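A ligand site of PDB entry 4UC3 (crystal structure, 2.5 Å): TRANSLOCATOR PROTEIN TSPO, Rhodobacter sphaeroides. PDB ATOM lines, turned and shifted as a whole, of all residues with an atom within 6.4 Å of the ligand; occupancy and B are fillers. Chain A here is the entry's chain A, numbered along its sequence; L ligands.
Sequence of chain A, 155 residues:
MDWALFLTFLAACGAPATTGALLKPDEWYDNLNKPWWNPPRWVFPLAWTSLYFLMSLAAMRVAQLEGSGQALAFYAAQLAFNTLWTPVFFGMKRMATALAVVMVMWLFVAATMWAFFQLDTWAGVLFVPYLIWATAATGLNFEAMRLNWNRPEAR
The indole nitrogen (NE1) of Trp 48 lies close to an oxygen (O5) of the ligand (2.9 Å). O5 of the ligand sits at hydrogen-bond distance from NE1 of Trp 133 (3.2 Å).
The side-chain hydroxyl (OG) of Ser 50 lies within hydrogen-bond range of the backbone carbonyl oxygen (O) of Leu 46, 2.8 Å away.
Pro 25 touches the ligand. Phe 44 touches the ligand. Ala 47 touches the ligand (CB to C10, 3.9 Å). Ser 50 touches the ligand. Leu 51 touches the ligand. Leu 54 touches the ligand (CD1 to C21, 3.4 Å). Pro 129 touches the ligand. CB of Ala 136 touches O3 of the ligand (3.7 Å). Hydrophobic or aromatic side chains within 4 Å of the ligand: Phe 44, Ala 47, Trp 48, Leu 51, Leu 54, Trp 133 and Ala 136. Of the 20 residues printed, 10 come within 4 Å of the ligand.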
ATOM      1  N   PRO A  25     -31.020 -25.752  -5.735  1.00  0.00           N
ATOM      2  CA  PRO A  25     -31.260 -24.382  -5.286  1.00  0.00           C
ATOM      3  C   PRO A  25     -31.366 -23.330  -6.400  1.00  0.00           C
ATOM      4  O   PRO A  25     -30.538 -23.405  -7.302  1.00  0.00           O
ATOM      5  CB  PRO A  25     -30.008 -24.083  -4.433  1.00  0.00           C
ATOM      6  CG  PRO A  25     -28.957 -25.172  -4.842  1.00  0.00           C
ATOM      7  CD  PRO A  25     -29.581 -25.991  -5.948  1.00  0.00           C
ATOM      8  N   ASP A  26     -32.321 -22.379  -6.393  1.00  0.00           N
ATOM      9  CA  ASP A  26     -33.401 -22.131  -5.412  1.00  0.00           C
ATOM     10  C   ASP A  26     -33.036 -22.234  -3.916  1.00  0.00           C
ATOM     11  O   ASP A  26     -33.736 -21.699  -3.042  1.00  0.00           O
ATOM     12  CB  ASP A  26     -34.581 -23.065  -5.711  1.00  0.00           C
ATOM     13  CG  ASP A  26     -35.798 -22.730  -4.874  1.00  0.00           C
ATOM     14  OD1 ASP A  26     -36.256 -21.562  -4.933  1.00  0.00           O
ATOM     15  OD2 ASP A  26     -36.294 -23.622  -4.156  1.00  0.00           O
ATOM     16  N   VAL A  43     -29.203 -22.454 -17.588  1.00  0.00           N
ATOM     17  CA  VAL A  43     -28.290 -21.444 -17.007  1.00  0.00           C
ATOM     18  C   VAL A  43     -27.501 -21.939 -15.762  1.00  0.00           C
ATOM     19  O   VAL A  43     -26.275 -21.787 -15.719  1.00  0.00           O
ATOM     20  CB  VAL A  43     -29.074 -20.138 -16.628  1.00  0.00           C
ATOM     21  CG1 VAL A  43     -28.198 -19.182 -15.863  1.00  0.00           C
ATOM     22  CG2 VAL A  43     -29.606 -19.459 -17.872  1.00  0.00           C
ATOM     23  N   PHE A  44     -28.179 -22.548 -14.805  1.00  0.00           N
ATOM     24  CA  PHE A  44     -27.569 -23.020 -13.552  1.00  0.00           C
ATOM     25  C   PHE A  44     -26.463 -24.060 -13.772  1.00  0.00           C
ATOM     26  O   PHE A  44     -25.325 -23.840 -13.336  1.00  0.00           O
ATOM     27  CB  PHE A  44     -28.656 -23.577 -12.613  1.00  0.00           C
ATOM     28  CG  PHE A  44     -28.153 -24.146 -11.300  1.00  0.00           C
ATOM     29  CD1 PHE A  44     -27.731 -23.317 -10.274  1.00  0.00           C
ATOM     30  CD2 PHE A  44     -28.156 -25.523 -11.081  1.00  0.00           C
ATOM     31  CE1 PHE A  44     -27.290 -23.852  -9.058  1.00  0.00           C
ATOM     32  CE2 PHE A  44     -27.715 -26.059  -9.865  1.00  0.00           C
ATOM     33  CZ  PHE A  44     -27.287 -25.227  -8.856  1.00  0.00           C
ATOM     34  N   LEU A  46     -24.998 -24.747 -16.570  1.00  0.00           N
ATOM     35  CA  LEU A  46     -24.033 -24.142 -17.476  1.00  0.00           C
ATOM     36  C   LEU A  46     -23.132 -23.198 -16.705  1.00  0.00           C
ATOM     37  O   LEU A  46     -21.936 -23.154 -16.935  1.00  0.00           O
ATOM     38  CB  LEU A  46     -24.715 -23.383 -18.619  1.00  0.00           C
ATOM     39  CG  LEU A  46     -23.818 -22.363 -19.339  1.00  0.00           C
ATOM     40  CD1 LEU A  46     -22.595 -23.031 -20.013  1.00  0.00           C
ATOM     41  CD2 LEU A  46     -24.604 -21.538 -20.335  1.00  0.00           C
ATOM     42  N   ALA A  47     -23.721 -22.432 -15.807  1.00  0.00           N
ATOM     43  CA  ALA A  47     -22.928 -21.530 -14.956  1.00  0.00           C
ATOM     44  C   ALA A  47     -21.934 -22.324 -14.098  1.00  0.00           C
ATOM     45  O   ALA A  47     -20.779 -21.905 -13.953  1.00  0.00           O
ATOM     46  CB  ALA A  47     -23.846 -20.702 -14.084  1.00  0.00           C
ATOM     47  N   TRP A  48     -22.381 -23.450 -13.546  1.00  0.00           N
ATOM     48  CA  TRP A  48     -21.551 -24.303 -12.705  1.00  0.00           C
ATOM     49  C   TRP A  48     -20.473 -25.132 -13.417  1.00  0.00           C
ATOM     50  O   TRP A  48     -19.336 -25.248 -12.920  1.00  0.00           O
ATOM     51  CB  TRP A  48     -22.444 -25.233 -11.891  1.00  0.00           C
ATOM     52  CG  TRP A  48     -22.874 -24.462 -10.758  1.00  0.00           C
ATOM     53  CD1 TRP A  48     -24.099 -23.912 -10.565  1.00  0.00           C
ATOM     54  CD2 TRP A  48     -22.066 -24.029  -9.669  1.00  0.00           C
ATOM     55  NE1 TRP A  48     -24.125 -23.196  -9.398  1.00  0.00           N
ATOM     56  CE2 TRP A  48     -22.870 -23.244  -8.819  1.00  0.00           C
ATOM     57  CE3 TRP A  48     -20.730 -24.253  -9.298  1.00  0.00           C
ATOM     58  CZ2 TRP A  48     -22.409 -22.686  -7.635  1.00  0.00           C
ATOM     59  CZ3 TRP A  48     -20.263 -23.693  -8.131  1.00  0.00           C
ATOM     60  CH2 TRP A  48     -21.092 -22.922  -7.304  1.00  0.00           C
ATOM     61  N   SER A  50     -19.010 -24.194 -16.101  1.00  0.00           N
ATOM     62  CA  SER A  50     -17.990 -23.196 -16.385  1.00  0.00           C
ATOM     63  C   SER A  50     -17.130 -22.976 -15.138  1.00  0.00           C
ATOM     64  O   SER A  50     -15.924 -23.012 -15.222  1.00  0.00           O
ATOM     65  CB  SER A  50     -18.640 -21.902 -16.850  1.00  0.00           C
ATOM     66  OG  SER A  50     -19.515 -22.149 -17.940  1.00  0.00           O
ATOM     67  N   LEU A  51     -17.757 -22.787 -13.982  1.00  0.00           N
ATOM     68  CA  LEU A  51     -17.020 -22.522 -12.740  1.00  0.00           C
ATOM     69  C   LEU A  51     -16.089 -23.683 -12.366  1.00  0.00           C
ATOM     70  O   LEU A  51     -14.926 -23.481 -11.998  1.00  0.00           O
ATOM     71  CB  LEU A  51     -17.974 -22.276 -11.566  1.00  0.00           C
ATOM     72  CG  LEU A  51     -18.856 -21.023 -11.562  1.00  0.00           C
ATOM     73  CD1 LEU A  51     -19.585 -20.879 -10.232  1.00  0.00           C
ATOM     74  CD2 LEU A  51     -18.081 -19.746 -11.951  1.00  0.00           C
ATOM     75  N   PHE A  53     -14.838 -25.874 -14.408  1.00  0.00           N
ATOM     76  CA  PHE A  53     -13.786 -25.991 -15.430  1.00  0.00           C
ATOM     77  C   PHE A  53     -12.710 -24.913 -15.170  1.00  0.00           C
ATOM     78  O   PHE A  53     -11.499 -25.209 -15.101  1.00  0.00           O
ATOM     79  CB  PHE A  53     -14.431 -25.898 -16.845  1.00  0.00           C
ATOM     80  CG  PHE A  53     -13.449 -25.710 -17.969  1.00  0.00           C
ATOM     81  CD1 PHE A  53     -12.499 -26.679 -18.265  1.00  0.00           C
ATOM     82  CD2 PHE A  53     -13.503 -24.565 -18.773  1.00  0.00           C
ATOM     83  CE1 PHE A  53     -11.594 -26.498 -19.330  1.00  0.00           C
ATOM     84  CE2 PHE A  53     -12.609 -24.372 -19.834  1.00  0.00           C
ATOM     85  CZ  PHE A  53     -11.664 -25.337 -20.106  1.00  0.00           C
ATOM     86  N   LEU A  54     -13.167 -23.682 -14.965  1.00  0.00           N
ATOM     87  CA  LEU A  54     -12.268 -22.554 -14.680  1.00  0.00           C
ATOM     88  C   LEU A  54     -11.373 -22.827 -13.469  1.00  0.00           C
ATOM     89  O   LEU A  54     -10.157 -22.551 -13.516  1.00  0.00           O
ATOM     90  CB  LEU A  54     -13.075 -21.285 -14.437  1.00  0.00           C
ATOM     91  CG  LEU A  54     -13.809 -20.684 -15.623  1.00  0.00           C
ATOM     92  CD1 LEU A  54     -14.676 -19.546 -15.167  1.00  0.00           C
ATOM     93  CD2 LEU A  54     -12.820 -20.206 -16.650  1.00  0.00           C
ATOM     94  N   TRP A  85     -21.483 -25.960   2.381  1.00  0.00           N
ATOM     95  CA  TRP A  85     -22.420 -24.861   2.485  1.00  0.00           C
ATOM     96  C   TRP A  85     -23.830 -25.234   2.011  1.00  0.00           C
ATOM     97  O   TRP A  85     -24.807 -24.995   2.718  1.00  0.00           O
ATOM     98  CB  TRP A  85     -21.942 -23.649   1.710  1.00  0.00           C
ATOM     99  CG  TRP A  85     -22.948 -22.572   1.816  1.00  0.00           C
ATOM    100  CD1 TRP A  85     -23.334 -21.949   2.961  1.00  0.00           C
ATOM    101  CD2 TRP A  85     -23.762 -22.037   0.767  1.00  0.00           C
ATOM    102  NE1 TRP A  85     -24.320 -21.033   2.687  1.00  0.00           N
ATOM    103  CE2 TRP A  85     -24.602 -21.068   1.348  1.00  0.00           C
ATOM    104  CE3 TRP A  85     -23.846 -22.277  -0.602  1.00  0.00           C
ATOM    105  CZ2 TRP A  85     -25.524 -20.343   0.604  1.00  0.00           C
ATOM    106  CZ3 TRP A  85     -24.756 -21.558  -1.343  1.00  0.00           C
ATOM    107  CH2 TRP A  85     -25.589 -20.598  -0.742  1.00  0.00           C
ATOM    108  N   PHE A  90     -29.457 -25.214   2.371  1.00  0.00           N
ATOM    109  CA  PHE A  90     -30.627 -25.698   1.649  1.00  0.00           C
ATOM    110  C   PHE A  90     -31.083 -27.030   2.179  1.00  0.00           C
ATOM    111  O   PHE A  90     -32.235 -27.401   1.992  1.00  0.00           O
ATOM    112  CB  PHE A  90     -30.351 -25.805   0.136  1.00  0.00           C
ATOM    113  CG  PHE A  90     -29.918 -24.514  -0.501  1.00  0.00           C
ATOM    114  CD1 PHE A  90     -30.856 -23.616  -0.953  1.00  0.00           C
ATOM    115  CD2 PHE A  90     -28.570 -24.218  -0.666  1.00  0.00           C
ATOM    116  CE1 PHE A  90     -30.470 -22.421  -1.541  1.00  0.00           C
ATOM    117  CE2 PHE A  90     -28.165 -23.041  -1.267  1.00  0.00           C
ATOM    118  CZ  PHE A  90     -29.119 -22.133  -1.699  1.00  0.00           C
ATOM    119  N   PRO A 129     -14.547 -15.080 -11.406  1.00  0.00           N
ATOM    120  CA  PRO A 129     -15.995 -15.318 -11.460  1.00  0.00           C
ATOM    121  C   PRO A 129     -16.536 -16.211 -10.337  1.00  0.00           C
ATOM    122  O   PRO A 129     -17.735 -16.137 -10.022  1.00  0.00           O
ATOM    123  CB  PRO A 129     -16.205 -15.988 -12.813  1.00  0.00           C
ATOM    124  CG  PRO A 129     -15.042 -15.567 -13.622  1.00  0.00           C
ATOM    125  CD  PRO A 129     -13.897 -15.446 -12.680  1.00  0.00           C
ATOM    126  N   TYR A 130     -15.662 -16.984  -9.716  1.00  0.00           N
ATOM    127  CA  TYR A 130     -16.058 -17.871  -8.635  1.00  0.00           C
ATOM    128  C   TYR A 130     -16.136 -17.105  -7.330  1.00  0.00           C
ATOM    129  O   TYR A 130     -17.005 -17.361  -6.511  1.00  0.00           O
ATOM    130  CB  TYR A 130     -15.078 -19.018  -8.533  1.00  0.00           C
ATOM    131  CG  TYR A 130     -15.373 -20.044  -7.456  1.00  0.00           C
ATOM    132  CD1 TYR A 130     -16.673 -20.456  -7.175  1.00  0.00           C
ATOM    133  CD2 TYR A 130     -14.334 -20.624  -6.748  1.00  0.00           C
ATOM    134  CE1 TYR A 130     -16.921 -21.415  -6.202  1.00  0.00           C
ATOM    135  CE2 TYR A 130     -14.566 -21.573  -5.786  1.00  0.00           C
ATOM    136  CZ  TYR A 130     -15.850 -21.975  -5.516  1.00  0.00           C
ATOM    137  OH  TYR A 130     -16.030 -22.919  -4.554  1.00  0.00           O
ATOM    138  N   ILE A 132     -17.120 -14.164  -7.355  1.00  0.00           N
ATOM    139  CA  ILE A 132     -18.366 -13.461  -7.580  1.00  0.00           C
ATOM    140  C   ILE A 132     -19.549 -14.322  -7.134  1.00  0.00           C
ATOM    141  O   ILE A 132     -20.440 -13.829  -6.445  1.00  0.00           O
ATOM    142  CB  ILE A 132     -18.490 -13.037  -9.030  1.00  0.00           C
ATOM    143  CG1 ILE A 132     -17.559 -11.839  -9.272  1.00  0.00           C
ATOM    144  CG2 ILE A 132     -19.919 -12.670  -9.362  1.00  0.00           C
ATOM    145  CD1 ILE A 132     -17.430 -11.373 -10.732  1.00  0.00           C
ATOM    146  N   TRP A 133     -19.581 -15.607  -7.505  1.00  0.00           N
ATOM    147  CA  TRP A 133     -20.607 -16.472  -6.949  1.00  0.00           C
ATOM    148  C   TRP A 133     -20.581 -16.530  -5.411  1.00  0.00           C
ATOM    149  O   TRP A 133     -21.626 -16.554  -4.773  1.00  0.00           O
ATOM    150  CB  TRP A 133     -20.516 -17.905  -7.479  1.00  0.00           C
ATOM    151  CG  TRP A 133     -21.400 -18.793  -6.649  1.00  0.00           C
ATOM    152  CD1 TRP A 133     -22.761 -18.877  -6.729  1.00  0.00           C
ATOM    153  CD2 TRP A 133     -21.006 -19.654  -5.572  1.00  0.00           C
ATOM    154  NE1 TRP A 133     -23.237 -19.771  -5.788  1.00  0.00           N
ATOM    155  CE2 TRP A 133     -22.173 -20.257  -5.057  1.00  0.00           C
ATOM    156  CE3 TRP A 133     -19.777 -19.984  -5.001  1.00  0.00           C
ATOM    157  CZ2 TRP A 133     -22.148 -21.174  -4.019  1.00  0.00           C
ATOM    158  CZ3 TRP A 133     -19.752 -20.901  -3.963  1.00  0.00           C
ATOM    159  CH2 TRP A 133     -20.931 -21.480  -3.479  1.00  0.00           C
ATOM    160  N   ALA A 136     -22.207 -13.713  -3.999  1.00  0.00           N
ATOM    161  CA  ALA A 136     -23.635 -13.876  -4.133  1.00  0.00           C
ATOM    162  C   ALA A 136     -24.188 -14.762  -3.014  1.00  0.00           C
ATOM    163  O   ALA A 136     -25.212 -14.480  -2.415  1.00  0.00           O
ATOM    164  CB  ALA A 136     -23.951 -14.470  -5.494  1.00  0.00           C
ATOM    165  N   ALA A 137     -23.479 -15.847  -2.763  1.00  0.00           N
ATOM    166  CA  ALA A 137     -23.853 -16.850  -1.772  1.00  0.00           C
ATOM    167  C   ALA A 137     -23.924 -16.264  -0.381  1.00  0.00           C
ATOM    168  O   ALA A 137     -24.849 -16.534   0.380  1.00  0.00           O
ATOM    169  CB  ALA A 137     -22.842 -18.004  -1.827  1.00  0.00           C
ATOM    170  N   LEU A 140     -26.992 -13.665  -0.203  1.00  0.00           N
ATOM    171  CA  LEU A 140     -28.249 -14.392  -0.071  1.00  0.00           C
ATOM    172  C   LEU A 140     -28.415 -14.886   1.353  1.00  0.00           C
ATOM    173  O   LEU A 140     -29.497 -14.843   1.927  1.00  0.00           O
ATOM    174  CB  LEU A 140     -28.310 -15.567  -1.060  1.00  0.00           C
ATOM    175  CG  LEU A 140     -29.408 -16.611  -0.816  1.00  0.00           C
ATOM    176  CD1 LEU A 140     -30.695 -16.194  -1.517  1.00  0.00           C
ATOM    177  CD2 LEU A 140     -29.005 -17.996  -1.291  1.00  0.00           C
HETATM  178  O1  LIG L   1     -29.311 -19.694  -6.711  1.00  0.00           O
HETATM  179  C1  LIG L   1     -28.506 -19.008  -7.661  1.00  0.00           C
HETATM  180  C2  LIG L   1     -27.423 -18.206  -6.983  1.00  0.00           C
HETATM  181  O2  LIG L   1     -26.397 -17.837  -7.898  1.00  0.00           O
HETATM  182  C3  LIG L   1     -26.539 -16.662  -8.741  1.00  0.00           C
HETATM  183  O3  LIG L   1     -25.897 -15.653  -8.458  1.00  0.00           O
HETATM  184  C4  LIG L   1     -27.446 -16.669 -10.016  1.00  0.00           C
HETATM  185  C5  LIG L   1     -27.153 -17.842 -11.010  1.00  0.00           C
HETATM  186  C6  LIG L   1     -26.791 -19.094  -5.896  1.00  0.00           C
HETATM  187  O4  LIG L   1     -26.911 -20.502  -6.267  1.00  0.00           O
HETATM  188  C7  LIG L   1     -26.056 -21.019  -7.287  1.00  0.00           C
HETATM  189  O5  LIG L   1     -25.295 -21.952  -7.001  1.00  0.00           O
HETATM  190  C8  LIG L   1     -26.070 -20.439  -8.755  1.00  0.00           C
HETATM  191  C9  LIG L   1     -24.661 -20.366  -9.414  1.00  0.00           C
HETATM  192  C10 LIG L   1     -24.458 -19.281 -10.526  1.00  0.00           C
HETATM  193  C11 LIG L   1     -23.361 -18.317 -10.134  1.00  0.00           C
HETATM  194  C12 LIG L   1     -22.878 -17.433 -11.358  1.00  0.00           C
HETATM  195  C13 LIG L   1     -21.809 -16.387 -10.951  1.00  0.00           C
HETATM  196  C14 LIG L   1     -20.383 -16.692 -11.543  1.00  0.00           C
HETATM  197  C15 LIG L   1     -20.312 -16.496 -13.082  1.00  0.00           C
HETATM  198  C16 LIG L   1     -20.125 -17.819 -13.852  1.00  0.00           C
HETATM  199  C17 LIG L   1     -19.903 -17.605 -15.404  1.00  0.00           C
HETATM  200  C18 LIG L   1     -18.537 -18.043 -15.901  1.00  0.00           C
HETATM  201  C19 LIG L   1     -17.796 -16.926 -16.796  1.00  0.00           C
HETATM  202  C20 LIG L   1     -17.240 -17.489 -18.125  1.00  0.00           C
HETATM  203  C21 LIG L   1     -15.782 -18.044 -18.008  1.00  0.00           C
HETATM  204  C22 LIG L   1     -15.638 -19.511 -18.438  1.00  0.00           C
HETATM  205  C23 LIG L   1     -15.209 -19.643 -19.902  1.00  0.00           C
HETATM  206  C24 LIG L   1     -15.726 -18.476 -20.703  1.00  0.00           C
